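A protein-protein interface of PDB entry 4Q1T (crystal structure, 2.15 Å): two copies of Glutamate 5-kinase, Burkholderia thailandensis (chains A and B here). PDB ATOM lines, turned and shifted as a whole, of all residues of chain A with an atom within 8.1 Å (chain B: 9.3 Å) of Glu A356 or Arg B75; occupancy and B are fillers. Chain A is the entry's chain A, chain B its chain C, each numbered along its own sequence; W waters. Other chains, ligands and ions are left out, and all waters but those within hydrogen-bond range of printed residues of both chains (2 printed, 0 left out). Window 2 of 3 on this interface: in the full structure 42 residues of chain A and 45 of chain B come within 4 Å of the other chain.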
ATOM      1  N   TYR A 339       3.090 -31.445  -3.464  1.00  0.00           N
ATOM      2  CA  TYR A 339       3.647 -30.347  -4.226  1.00  0.00           C
ATOM      3  C   TYR A 339       5.163 -30.337  -4.137  1.00  0.00           C
ATOM      4  O   TYR A 339       5.735 -30.789  -3.144  1.00  0.00           O
ATOM      5  CB  TYR A 339       3.104 -29.016  -3.689  1.00  0.00           C
ATOM      6  CG  TYR A 339       1.633 -28.778  -4.014  1.00  0.00           C
ATOM      7  CD1 TYR A 339       1.250 -28.243  -5.225  1.00  0.00           C
ATOM      8  CD2 TYR A 339       0.628 -29.121  -3.116  1.00  0.00           C
ATOM      9  CE1 TYR A 339      -0.098 -28.034  -5.528  1.00  0.00           C
ATOM     10  CE2 TYR A 339      -0.713 -28.902  -3.407  1.00  0.00           C
ATOM     11  CZ  TYR A 339      -1.071 -28.369  -4.619  1.00  0.00           C
ATOM     12  OH  TYR A 339      -2.408 -28.163  -4.949  1.00  0.00           O
ATOM     13  N   ILE A 347       2.764 -21.111  -2.714  1.00  0.00           N
ATOM     14  CA  ILE A 347       1.434 -21.224  -2.120  1.00  0.00           C
ATOM     15  C   ILE A 347       1.457 -21.259  -0.611  1.00  0.00           C
ATOM     16  O   ILE A 347       0.398 -21.343   0.027  1.00  0.00           O
ATOM     17  CB  ILE A 347       0.669 -22.458  -2.659  1.00  0.00           C
ATOM     18  CG1 ILE A 347       1.307 -23.760  -2.162  1.00  0.00           C
ATOM     19  CG2 ILE A 347       0.608 -22.406  -4.179  1.00  0.00           C
ATOM     20  CD1 ILE A 347       0.548 -25.009  -2.551  1.00  0.00           C
ATOM     21  N   PRO A 351      -4.799 -19.793   1.464  1.00  0.00           N
ATOM     22  CA  PRO A 351      -5.903 -20.745   1.555  1.00  0.00           C
ATOM     23  C   PRO A 351      -5.987 -21.567   0.268  1.00  0.00           C
ATOM     24  O   PRO A 351      -5.527 -21.116  -0.782  1.00  0.00           O
ATOM     25  CB  PRO A 351      -7.157 -19.855   1.716  1.00  0.00           C
ATOM     26  CG  PRO A 351      -6.654 -18.465   1.976  1.00  0.00           C
ATOM     27  CD  PRO A 351      -5.277 -18.398   1.375  1.00  0.00           C
ATOM     28  N   SER A 352      -6.574 -22.751   0.352  1.00  0.00           N
ATOM     29  CA  SER A 352      -6.593 -23.680  -0.774  1.00  0.00           C
ATOM     30  C   SER A 352      -7.297 -23.137  -2.016  1.00  0.00           C
ATOM     31  O   SER A 352      -6.855 -23.398  -3.142  1.00  0.00           O
ATOM     32  CB  SER A 352      -7.238 -25.002  -0.358  1.00  0.00           C
ATOM     33  OG  SER A 352      -6.379 -25.658   0.570  1.00  0.00           O
ATOM     34  N   GLY A 353      -8.348 -22.346  -1.815  1.00  0.00           N
ATOM     35  CA  GLY A 353      -9.051 -21.734  -2.927  1.00  0.00           C
ATOM     36  C   GLY A 353      -8.232 -20.710  -3.711  1.00  0.00           C
ATOM     37  O   GLY A 353      -8.664 -20.267  -4.781  1.00  0.00           O
ATOM     38  N   GLU A 354      -7.074 -20.303  -3.183  1.00  0.00           N
ATOM     39  CA  GLU A 354      -6.190 -19.375  -3.884  1.00  0.00           C
ATOM     40  C   GLU A 354      -5.043 -20.062  -4.641  1.00  0.00           C
ATOM     41  O   GLU A 354      -4.329 -19.399  -5.406  1.00  0.00           O
ATOM     42  CB  GLU A 354      -5.622 -18.333  -2.913  1.00  0.00           C
ATOM     43  CG  GLU A 354      -6.646 -17.326  -2.420  1.00  0.00           C
ATOM     44  CD  GLU A 354      -6.062 -16.295  -1.454  1.00  0.00           C
ATOM     45  OE1 GLU A 354      -4.819 -16.127  -1.416  1.00  0.00           O
ATOM     46  OE2 GLU A 354      -6.853 -15.644  -0.727  1.00  0.00           O
ATOM     47  N   ILE A 355      -4.861 -21.371  -4.450  1.00  0.00           N
ATOM     48  CA  ILE A 355      -3.764 -22.096  -5.115  1.00  0.00           C
ATOM     49  C   ILE A 355      -3.825 -22.015  -6.634  1.00  0.00           C
ATOM     50  O   ILE A 355      -2.796 -21.822  -7.272  1.00  0.00           O
ATOM     51  CB  ILE A 355      -3.734 -23.592  -4.748  1.00  0.00           C
ATOM     52  CG1 ILE A 355      -3.327 -23.768  -3.298  1.00  0.00           C
ATOM     53  CG2 ILE A 355      -2.736 -24.347  -5.629  1.00  0.00           C
ATOM     54  CD1 ILE A 355      -3.628 -25.153  -2.784  1.00  0.00           C
ATOM     55  N   GLU A 356      -5.027 -22.162  -7.202  1.00  0.00           N
ATOM     56  CA  GLU A 356      -5.202 -22.170  -8.655  1.00  0.00           C
ATOM     57  C   GLU A 356      -4.761 -20.865  -9.324  1.00  0.00           C
ATOM     58  O   GLU A 356      -4.083 -20.891 -10.356  1.00  0.00           O
ATOM     59  CB  GLU A 356      -6.652 -22.476  -9.028  1.00  0.00           C
ATOM     60  CG  GLU A 356      -6.860 -22.611 -10.535  1.00  0.00           C
ATOM     61  CD  GLU A 356      -7.980 -23.571 -10.924  1.00  0.00           C
ATOM     62  OE1 GLU A 356      -8.804 -23.944 -10.065  1.00  0.00           O
ATOM     63  OE2 GLU A 356      -8.030 -23.944 -12.110  1.00  0.00           O
ATOM     64  N   ALA A 357      -5.135 -19.734  -8.728  1.00  0.00           N
ATOM     65  CA  ALA A 357      -4.712 -18.417  -9.215  1.00  0.00           C
ATOM     66  C   ALA A 357      -3.195 -18.240  -9.159  1.00  0.00           C
ATOM     67  O   ALA A 357      -2.602 -17.687 -10.084  1.00  0.00           O
ATOM     68  CB  ALA A 357      -5.388 -17.313  -8.423  1.00  0.00           C
ATOM     69  N   VAL A 358      -2.572 -18.705  -8.080  1.00  0.00           N
ATOM     70  CA  VAL A 358      -1.134 -18.519  -7.893  1.00  0.00           C
ATOM     71  C   VAL A 358      -0.316 -19.372  -8.854  1.00  0.00           C
ATOM     72  O   VAL A 358       0.641 -18.878  -9.454  1.00  0.00           O
ATOM     73  CB  VAL A 358      -0.699 -18.827  -6.440  1.00  0.00           C
ATOM     74  CG1 VAL A 358       0.822 -18.877  -6.323  1.00  0.00           C
ATOM     75  CG2 VAL A 358      -1.274 -17.779  -5.494  1.00  0.00           C
ATOM     76  N   LEU A 359      -0.684 -20.647  -9.002  1.00  0.00           N
ATOM     77  CA  LEU A 359       0.089 -21.576  -9.821  1.00  0.00           C
ATOM     78  C   LEU A 359      -0.340 -21.627 -11.288  1.00  0.00           C
ATOM     79  O   LEU A 359       0.460 -22.018 -12.141  1.00  0.00           O
ATOM     80  CB  LEU A 359       0.014 -22.993  -9.228  1.00  0.00           C
ATOM     81  CG  LEU A 359       0.672 -23.215  -7.875  1.00  0.00           C
ATOM     82  CD1 LEU A 359       0.583 -24.686  -7.502  1.00  0.00           C
ATOM     83  CD2 LEU A 359       2.119 -22.716  -7.863  1.00  0.00           C
ATOM     84  N   GLY A 360      -1.603 -21.294 -11.572  1.00  0.00           N
ATOM     85  CA  GLY A 360      -2.200 -21.546 -12.886  1.00  0.00           C
ATOM     86  C   GLY A 360      -2.912 -22.897 -12.977  1.00  0.00           C
ATOM     87  O   GLY A 360      -3.504 -23.233 -14.010  1.00  0.00           O
ATOM     88  N   TYR A 361      -2.863 -23.671 -11.896  1.00  0.00           N
ATOM     89  CA  TYR A 361      -3.499 -24.989 -11.823  1.00  0.00           C
ATOM     90  C   TYR A 361      -3.537 -25.355 -10.352  1.00  0.00           C
ATOM     91  O   TYR A 361      -2.939 -24.662  -9.520  1.00  0.00           O
ATOM     92  CB  TYR A 361      -2.680 -26.057 -12.588  1.00  0.00           C
ATOM     93  CG  TYR A 361      -1.232 -26.127 -12.135  1.00  0.00           C
ATOM     94  CD1 TYR A 361      -0.285 -25.272 -12.661  1.00  0.00           C
ATOM     95  CD2 TYR A 361      -0.838 -27.005 -11.142  1.00  0.00           C
ATOM     96  CE1 TYR A 361       1.021 -25.303 -12.232  1.00  0.00           C
ATOM     97  CE2 TYR A 361       0.473 -27.049 -10.701  1.00  0.00           C
ATOM     98  CZ  TYR A 361       1.393 -26.192 -11.251  1.00  0.00           C
ATOM     99  OH  TYR A 361       2.699 -26.218 -10.837  1.00  0.00           O
ATOM    100  N   MET A 362      -4.225 -26.426 -10.006  1.00  0.00           N
ATOM    101  CA  MET A 362      -4.031 -26.979  -8.676  1.00  0.00           C
ATOM    102  C   MET A 362      -4.005 -28.476  -8.723  1.00  0.00           C
ATOM    103  O   MET A 362      -4.496 -29.094  -9.656  1.00  0.00           O
ATOM    104  CB  MET A 362      -5.080 -26.480  -7.683  1.00  0.00           C
ATOM    105  CG  MET A 362      -6.431 -27.149  -7.783  1.00  0.00           C
ATOM    106  SD  MET A 362      -7.530 -26.610  -6.491  1.00  0.00           S
ATOM    107  CE  MET A 362      -6.617 -26.974  -4.970  1.00  0.00           C
ATOM    108  N   LEU A 363      -3.390 -29.040  -7.698  1.00  0.00           N
ATOM    109  CA  LEU A 363      -3.372 -30.458  -7.502  1.00  0.00           C
ATOM    110  C   LEU A 363      -4.431 -30.757  -6.432  1.00  0.00           C
ATOM    111  O   LEU A 363      -5.593 -30.471  -6.659  1.00  0.00           O
ATOM    112  CB  LEU A 363      -1.945 -30.895  -7.151  1.00  0.00           C
ATOM    113  CG  LEU A 363      -0.893 -30.513  -8.210  1.00  0.00           C
ATOM    114  CD1 LEU A 363       0.474 -31.032  -7.780  1.00  0.00           C
ATOM    115  CD2 LEU A 363      -1.244 -31.054  -9.588  1.00  0.00           C
ATOM    116  N   GLU A 364      -4.040 -31.280  -5.268  1.00  0.00           N
ATOM    117  CA  GLU A 364      -4.943 -31.459  -4.114  1.00  0.00           C
ATOM    118  C   GLU A 364      -4.951 -30.195  -3.267  1.00  0.00           C
ATOM    119  O   GLU A 364      -4.035 -29.380  -3.370  1.00  0.00           O
ATOM    120  CB  GLU A 364      -4.491 -32.657  -3.254  1.00  0.00           C
ATOM    121  CG  GLU A 364      -4.568 -34.031  -3.941  1.00  0.00           C
ATOM    122  CD  GLU A 364      -3.302 -34.439  -4.705  1.00  0.00           C
ATOM    123  OE1 GLU A 364      -2.414 -33.569  -4.908  1.00  0.00           O
ATOM    124  OE2 GLU A 364      -3.192 -35.654  -5.069  1.00  0.00           O
ATOM    125  N   PRO A 365      -5.991 -30.004  -2.428  1.00  0.00           N
ATOM    126  CA  PRO A 365      -5.966 -28.849  -1.506  1.00  0.00           C
ATOM    127  C   PRO A 365      -4.927 -28.961  -0.366  1.00  0.00           C
ATOM    128  O   PRO A 365      -4.463 -27.945   0.159  1.00  0.00           O
ATOM    129  CB  PRO A 365      -7.397 -28.777  -0.940  1.00  0.00           C
ATOM    130  CG  PRO A 365      -8.075 -30.044  -1.322  1.00  0.00           C
ATOM    131  CD  PRO A 365      -7.263 -30.750  -2.386  1.00  0.00           C
ATOM    132  N   ILE B  61     -14.353 -38.194 -18.249  1.00  0.00           N
ATOM    133  CA  ILE B  61     -14.577 -37.295 -17.117  1.00  0.00           C
ATOM    134  C   ILE B  61     -16.023 -36.813 -17.079  1.00  0.00           C
ATOM    135  O   ILE B  61     -16.651 -36.804 -16.004  1.00  0.00           O
ATOM    136  CB  ILE B  61     -13.569 -36.129 -17.086  1.00  0.00           C
ATOM    137  CG1 ILE B  61     -12.234 -36.655 -16.583  1.00  0.00           C
ATOM    138  CG2 ILE B  61     -14.044 -34.999 -16.157  1.00  0.00           C
ATOM    139  CD1 ILE B  61     -11.063 -35.724 -16.834  1.00  0.00           C
ATOM    140  N   MET B  65     -18.591 -37.521 -14.121  1.00  0.00           N
ATOM    141  CA  MET B  65     -19.304 -36.418 -13.496  1.00  0.00           C
ATOM    142  C   MET B  65     -20.778 -36.765 -13.401  1.00  0.00           C
ATOM    143  O   MET B  65     -21.358 -36.671 -12.330  1.00  0.00           O
ATOM    144  CB  MET B  65     -19.136 -35.118 -14.287  1.00  0.00           C
ATOM    145  CG  MET B  65     -17.846 -34.369 -14.027  1.00  0.00           C
ATOM    146  SD  MET B  65     -17.519 -33.174 -15.355  1.00  0.00           S
ATOM    147  CE  MET B  65     -18.917 -32.049 -15.071  1.00  0.00           C
ATOM    148  N   TRP B  70     -22.220 -34.740 -10.340  1.00  0.00           N
ATOM    149  CA  TRP B  70     -21.548 -33.441 -10.402  1.00  0.00           C
ATOM    150  C   TRP B  70     -21.958 -32.674 -11.654  1.00  0.00           C
ATOM    151  O   TRP B  70     -21.853 -33.182 -12.763  1.00  0.00           O
ATOM    152  CB  TRP B  70     -20.031 -33.626 -10.405  1.00  0.00           C
ATOM    153  CG  TRP B  70     -19.471 -34.220  -9.151  1.00  0.00           C
ATOM    154  CD1 TRP B  70     -20.064 -34.266  -7.921  1.00  0.00           C
ATOM    155  CD2 TRP B  70     -18.189 -34.854  -9.001  1.00  0.00           C
ATOM    156  NE1 TRP B  70     -19.234 -34.878  -7.020  1.00  0.00           N
ATOM    157  CE2 TRP B  70     -18.079 -35.258  -7.655  1.00  0.00           C
ATOM    158  CE3 TRP B  70     -17.132 -35.115  -9.869  1.00  0.00           C
ATOM    159  CZ2 TRP B  70     -16.944 -35.898  -7.152  1.00  0.00           C
ATOM    160  CZ3 TRP B  70     -15.999 -35.761  -9.368  1.00  0.00           C
ATOM    161  CH2 TRP B  70     -15.927 -36.156  -8.017  1.00  0.00           C
ATOM    162  N   ARG B  72     -20.659 -29.442 -12.263  1.00  0.00           N
ATOM    163  CA  ARG B  72     -19.485 -28.645 -12.603  1.00  0.00           C
ATOM    164  C   ARG B  72     -18.214 -29.528 -12.623  1.00  0.00           C
ATOM    165  O   ARG B  72     -18.030 -30.415 -11.780  1.00  0.00           O
ATOM    166  CB  ARG B  72     -19.333 -27.484 -11.605  1.00  0.00           C
ATOM    167  N   ARG B  73     -17.372 -29.312 -13.632  1.00  0.00           N
ATOM    168  CA  ARG B  73     -16.106 -30.001 -13.732  1.00  0.00           C
ATOM    169  C   ARG B  73     -15.292 -29.677 -12.478  1.00  0.00           C
ATOM    170  O   ARG B  73     -15.114 -28.517 -12.135  1.00  0.00           O
ATOM    171  CB  ARG B  73     -15.369 -29.551 -14.988  1.00  0.00           C
ATOM    172  CG  ARG B  73     -14.145 -30.393 -15.328  1.00  0.00           C
ATOM    173  CD  ARG B  73     -13.456 -29.869 -16.571  1.00  0.00           C
ATOM    174  NE  ARG B  73     -12.060 -30.282 -16.641  1.00  0.00           N
ATOM    175  CZ  ARG B  73     -11.612 -31.327 -17.328  1.00  0.00           C
ATOM    176  NH1 ARG B  73     -12.444 -32.108 -18.020  1.00  0.00           N
ATOM    177  NH2 ARG B  73     -10.310 -31.586 -17.318  1.00  0.00           N
ATOM    178  N   PRO B  74     -14.817 -30.706 -11.773  1.00  0.00           N
ATOM    179  CA  PRO B  74     -14.051 -30.420 -10.553  1.00  0.00           C
ATOM    180  C   PRO B  74     -12.702 -29.776 -10.854  1.00  0.00           C
ATOM    181  O   PRO B  74     -12.141 -29.998 -11.918  1.00  0.00           O
ATOM    182  CB  PRO B  74     -13.850 -31.798  -9.927  1.00  0.00           C
ATOM    183  CG  PRO B  74     -14.006 -32.772 -11.047  1.00  0.00           C
ATOM    184  CD  PRO B  74     -14.890 -32.147 -12.083  1.00  0.00           C
ATOM    185  N   ARG B  75     -12.232 -28.955  -9.921  1.00  0.00           N
ATOM    186  CA  ARG B  75     -10.944 -28.285 -10.031  1.00  0.00           C
ATOM    187  C   ARG B  75      -9.822 -29.115  -9.448  1.00  0.00           C
ATOM    188  O   ARG B  75      -8.704 -29.044  -9.938  1.00  0.00           O
ATOM    189  CB  ARG B  75     -10.944 -26.952  -9.268  1.00  0.00           C
ATOM    190  CG  ARG B  75     -11.982 -25.943  -9.732  1.00  0.00           C
ATOM    191  CD  ARG B  75     -11.751 -25.482 -11.171  1.00  0.00           C
ATOM    192  NE  ARG B  75     -12.775 -24.500 -11.524  1.00  0.00           N
ATOM    193  CZ  ARG B  75     -12.690 -23.179 -11.343  1.00  0.00           C
ATOM    194  NH1 ARG B  75     -11.593 -22.605 -10.835  1.00  0.00           N
ATOM    195  NH2 ARG B  75     -13.720 -22.413 -11.695  1.00  0.00           N
ATOM    196  N   GLU B  76     -10.112 -29.852  -8.374  1.00  0.00           N
ATOM    197  CA  GLU B  76      -9.083 -30.659  -7.699  1.00  0.00           C
ATOM    198  C   GLU B  76      -8.758 -31.914  -8.476  1.00  0.00           C
ATOM    199  O   GLU B  76      -9.642 -32.570  -9.024  1.00  0.00           O
ATOM    200  CB  GLU B  76      -9.510 -31.037  -6.286  1.00  0.00           C
ATOM    201  CG  GLU B  76      -9.657 -29.839  -5.376  1.00  0.00           C
ATOM    202  CD  GLU B  76     -10.895 -29.873  -4.493  1.00  0.00           C
ATOM    203  OE1 GLU B  76     -11.621 -28.851  -4.411  1.00  0.00           O
ATOM    204  OE2 GLU B  76     -11.125 -30.925  -3.866  1.00  0.00           O
ATOM    205  N   ILE B  77      -7.470 -32.206  -8.589  1.00  0.00           N
ATOM    206  CA  ILE B  77      -7.008 -33.259  -9.489  1.00  0.00           C
ATOM    207  C   ILE B  77      -7.541 -34.638  -9.099  1.00  0.00           C
ATOM    208  O   ILE B  77      -7.852 -35.453  -9.964  1.00  0.00           O
ATOM    209  CB  ILE B  77      -5.453 -33.256  -9.591  1.00  0.00           C
ATOM    210  CG1 ILE B  77      -4.987 -34.020 -10.818  1.00  0.00           C
ATOM    211  CG2 ILE B  77      -4.770 -33.809  -8.348  1.00  0.00           C
ATOM    212  CD1 ILE B  77      -5.025 -33.164 -12.063  1.00  0.00           C
ATOM    213  N   ASP B  78      -7.616 -34.895  -7.800  1.00  0.00           N
ATOM    214  CA  ASP B  78      -8.068 -36.176  -7.302  1.00  0.00           C
ATOM    215  C   ASP B  78      -9.526 -36.417  -7.661  1.00  0.00           C
ATOM    216  O   ASP B  78      -9.871 -37.535  -8.034  1.00  0.00           O
ATOM    217  CB  ASP B  78      -7.843 -36.323  -5.797  1.00  0.00           C
ATOM    218  CG  ASP B  78      -8.435 -35.176  -4.991  1.00  0.00           C
ATOM    219  OD1 ASP B  78      -8.914 -34.178  -5.579  1.00  0.00           O
ATOM    220  OD2 ASP B  78      -8.395 -35.272  -3.761  1.00  0.00           O
ATOM    221  N   GLU B  79     -10.363 -35.375  -7.646  1.00  0.00           N
ATOM    222  CA  GLU B  79     -11.759 -35.528  -8.074  1.00  0.00           C
ATOM    223  C   GLU B  79     -11.848 -35.733  -9.565  1.00  0.00           C
ATOM    224  O   GLU B  79     -12.654 -36.527 -10.034  1.00  0.00           O
ATOM    225  CB  GLU B  79     -12.647 -34.371  -7.585  1.00  0.00           C
ATOM    226  CG  GLU B  79     -12.778 -34.414  -6.076  1.00  0.00           C
ATOM    227  CD  GLU B  79     -13.832 -33.486  -5.498  1.00  0.00           C
ATOM    228  OE1 GLU B  79     -14.237 -32.518  -6.167  1.00  0.00           O
ATOM    229  OE2 GLU B  79     -14.248 -33.750  -4.356  1.00  0.00           O
ATOM    230  N   LEU B  80     -10.970 -35.092 -10.324  1.00  0.00           N
ATOM    231  CA  LEU B  80     -10.874 -35.361 -11.751  1.00  0.00           C
ATOM    232  C   LEU B  80     -10.447 -36.801 -12.033  1.00  0.00           C
ATOM    233  O   LEU B  80     -10.991 -37.450 -12.913  1.00  0.00           O
ATOM    234  CB  LEU B  80      -9.925 -34.382 -12.434  1.00  0.00           C
ATOM    235  CG  LEU B  80     -10.440 -32.950 -12.609  1.00  0.00           C
ATOM    236  CD1 LEU B  80      -9.309 -32.028 -13.027  1.00  0.00           C
ATOM    237  CD2 LEU B  80     -11.538 -32.902 -13.659  1.00  0.00           C
ATOM    238  N   GLN B  81      -9.465 -37.307 -11.292  1.00  0.00           N
ATOM    239  CA  GLN B  81      -9.024 -38.675 -11.472  1.00  0.00           C
ATOM    240  C   GLN B  81     -10.145 -39.656 -11.132  1.00  0.00           C
ATOM    241  O   GLN B  81     -10.309 -40.662 -11.804  1.00  0.00           O
ATOM    242  CB  GLN B  81      -7.825 -38.973 -10.602  1.00  0.00           C
ATOM    243  CG  GLN B  81      -6.548 -38.277 -11.074  1.00  0.00           C
ATOM    244  CD  GLN B  81      -5.433 -38.478 -10.076  1.00  0.00           C
ATOM    245  OE1 GLN B  81      -5.513 -37.958  -8.974  1.00  0.00           O
ATOM    246  NE2 GLN B  81      -4.440 -39.274 -10.420  1.00  0.00           N
ATOM    247  N   ILE B 152      -4.629 -34.269 -18.025  1.00  0.00           N
ATOM    248  CA  ILE B 152      -5.995 -34.202 -17.545  1.00  0.00           C
ATOM    249  C   ILE B 152      -6.557 -32.803 -17.722  1.00  0.00           C
ATOM    250  O   ILE B 152      -7.710 -32.656 -18.134  1.00  0.00           O
ATOM    251  CB  ILE B 152      -6.125 -34.669 -16.048  1.00  0.00           C
ATOM    252  CG1 ILE B 152      -6.863 -36.012 -15.994  1.00  0.00           C
ATOM    253  CG2 ILE B 152      -6.832 -33.614 -15.180  1.00  0.00           C
ATOM    254  CD1 ILE B 152      -7.476 -36.398 -14.651  1.00  0.00           C
ATOM    255  N   LYS B 153      -5.740 -31.794 -17.420  1.00  0.00           N
ATOM    256  CA  LYS B 153      -6.175 -30.393 -17.393  1.00  0.00           C
ATOM    257  C   LYS B 153      -6.688 -29.900 -18.756  1.00  0.00           C
ATOM    258  O   LYS B 153      -7.857 -29.512 -18.886  1.00  0.00           O
ATOM    259  CB  LYS B 153      -5.037 -29.479 -16.906  1.00  0.00           C
HETATM  260  O   HOH W   1      -6.511 -30.017 -10.819  1.00  0.00           O
HETATM  261  O   HOH W   2      -3.489 -37.467  -7.216  1.00  0.00           O
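Arg B75 touches Met A362 (O to CG, 3.7 Å).
O of Leu A363 touches CA of Glu B76 (3.6 Å).
Ile B77 touches Glu A364 (CG2 to CD, 3.98 Å).
Glu B76 touches Pro A365.
No position is printed for both chains.
Of the 6 pairs that touch across the chains among the printed residues, none has its exchanged pair printed and touching as well.
Of the 17 printed residues of chain A, 5 touch a printed residue of chain B.
Hydrophobic or aromatic side chains of chain A that line the printed part of chain B: Met A362 and Pro A365.
Hydrophobic or aromatic side chains of chain B that line the printed part of chain A: Ile B77.
Among the printed residues, Asp or Glu carboxylates within 4 Å of a Lys or Arg side-chain nitrogen of the other chain: Glu A356 with Arg B75 (3.2 Å).
OH of Tyr A339 sits at hydrogen-bond distance from N of Leu A363 (3.0 Å).
The backbone NH of Tyr A361 lies within hydrogen-bond range of the backbone carbonyl oxygen of Glu A356 (3.4 Å).
The side-chain hydroxyl of Ser A352 lies within hydrogen-bond range of the backbone carbonyl oxygen of Pro A365, 3.0 Å away.
O of Glu A364 sits at hydrogen-bond distance from OH of Tyr A339 (2.6 Å).
O of Leu A363 sits at hydrogen-bond distance from N of Ile B77 (3.2 Å).
The side-chain carboxylate (OE1) of Glu A356 is in salt-bridge range of the guanidinium group (NH1) of Arg B75 (3.2 Å).
Of chain B, only Arg B75 (3.2 Å) comes within 4 Å of Glu A356.
No residue of chain B comes within 4 Å of Ala A357.
Of the printed residues of chain B, Met A362 touches Arg B75 (3.7 Å).
Of the printed residues of chain B, Leu A363 touches Glu B76 (3.6 Å) and Ile B77 (3.2 Å).
Printed residues of chain B within 4 Å of Pro A365: Glu B76 (3.9 Å).
The nearest residue of chain A that does not touch Arg B75 is Leu A363 (4.7 Å).
The nearest printed residue of chain B that does not touch Glu A364 is Asp B78 (4.03 Å).
Water W1 lies within hydrogen-bond range of the backbone carbonyl oxygen of Met A362 (2.5 Å), the backbone carbonyl oxygen of Arg B75 (2.6 Å) and the backbone NH of Ile B77 (3.3 Å).
Water W2 bridges OE1 of Gln B81 and OE2 of Glu A364.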
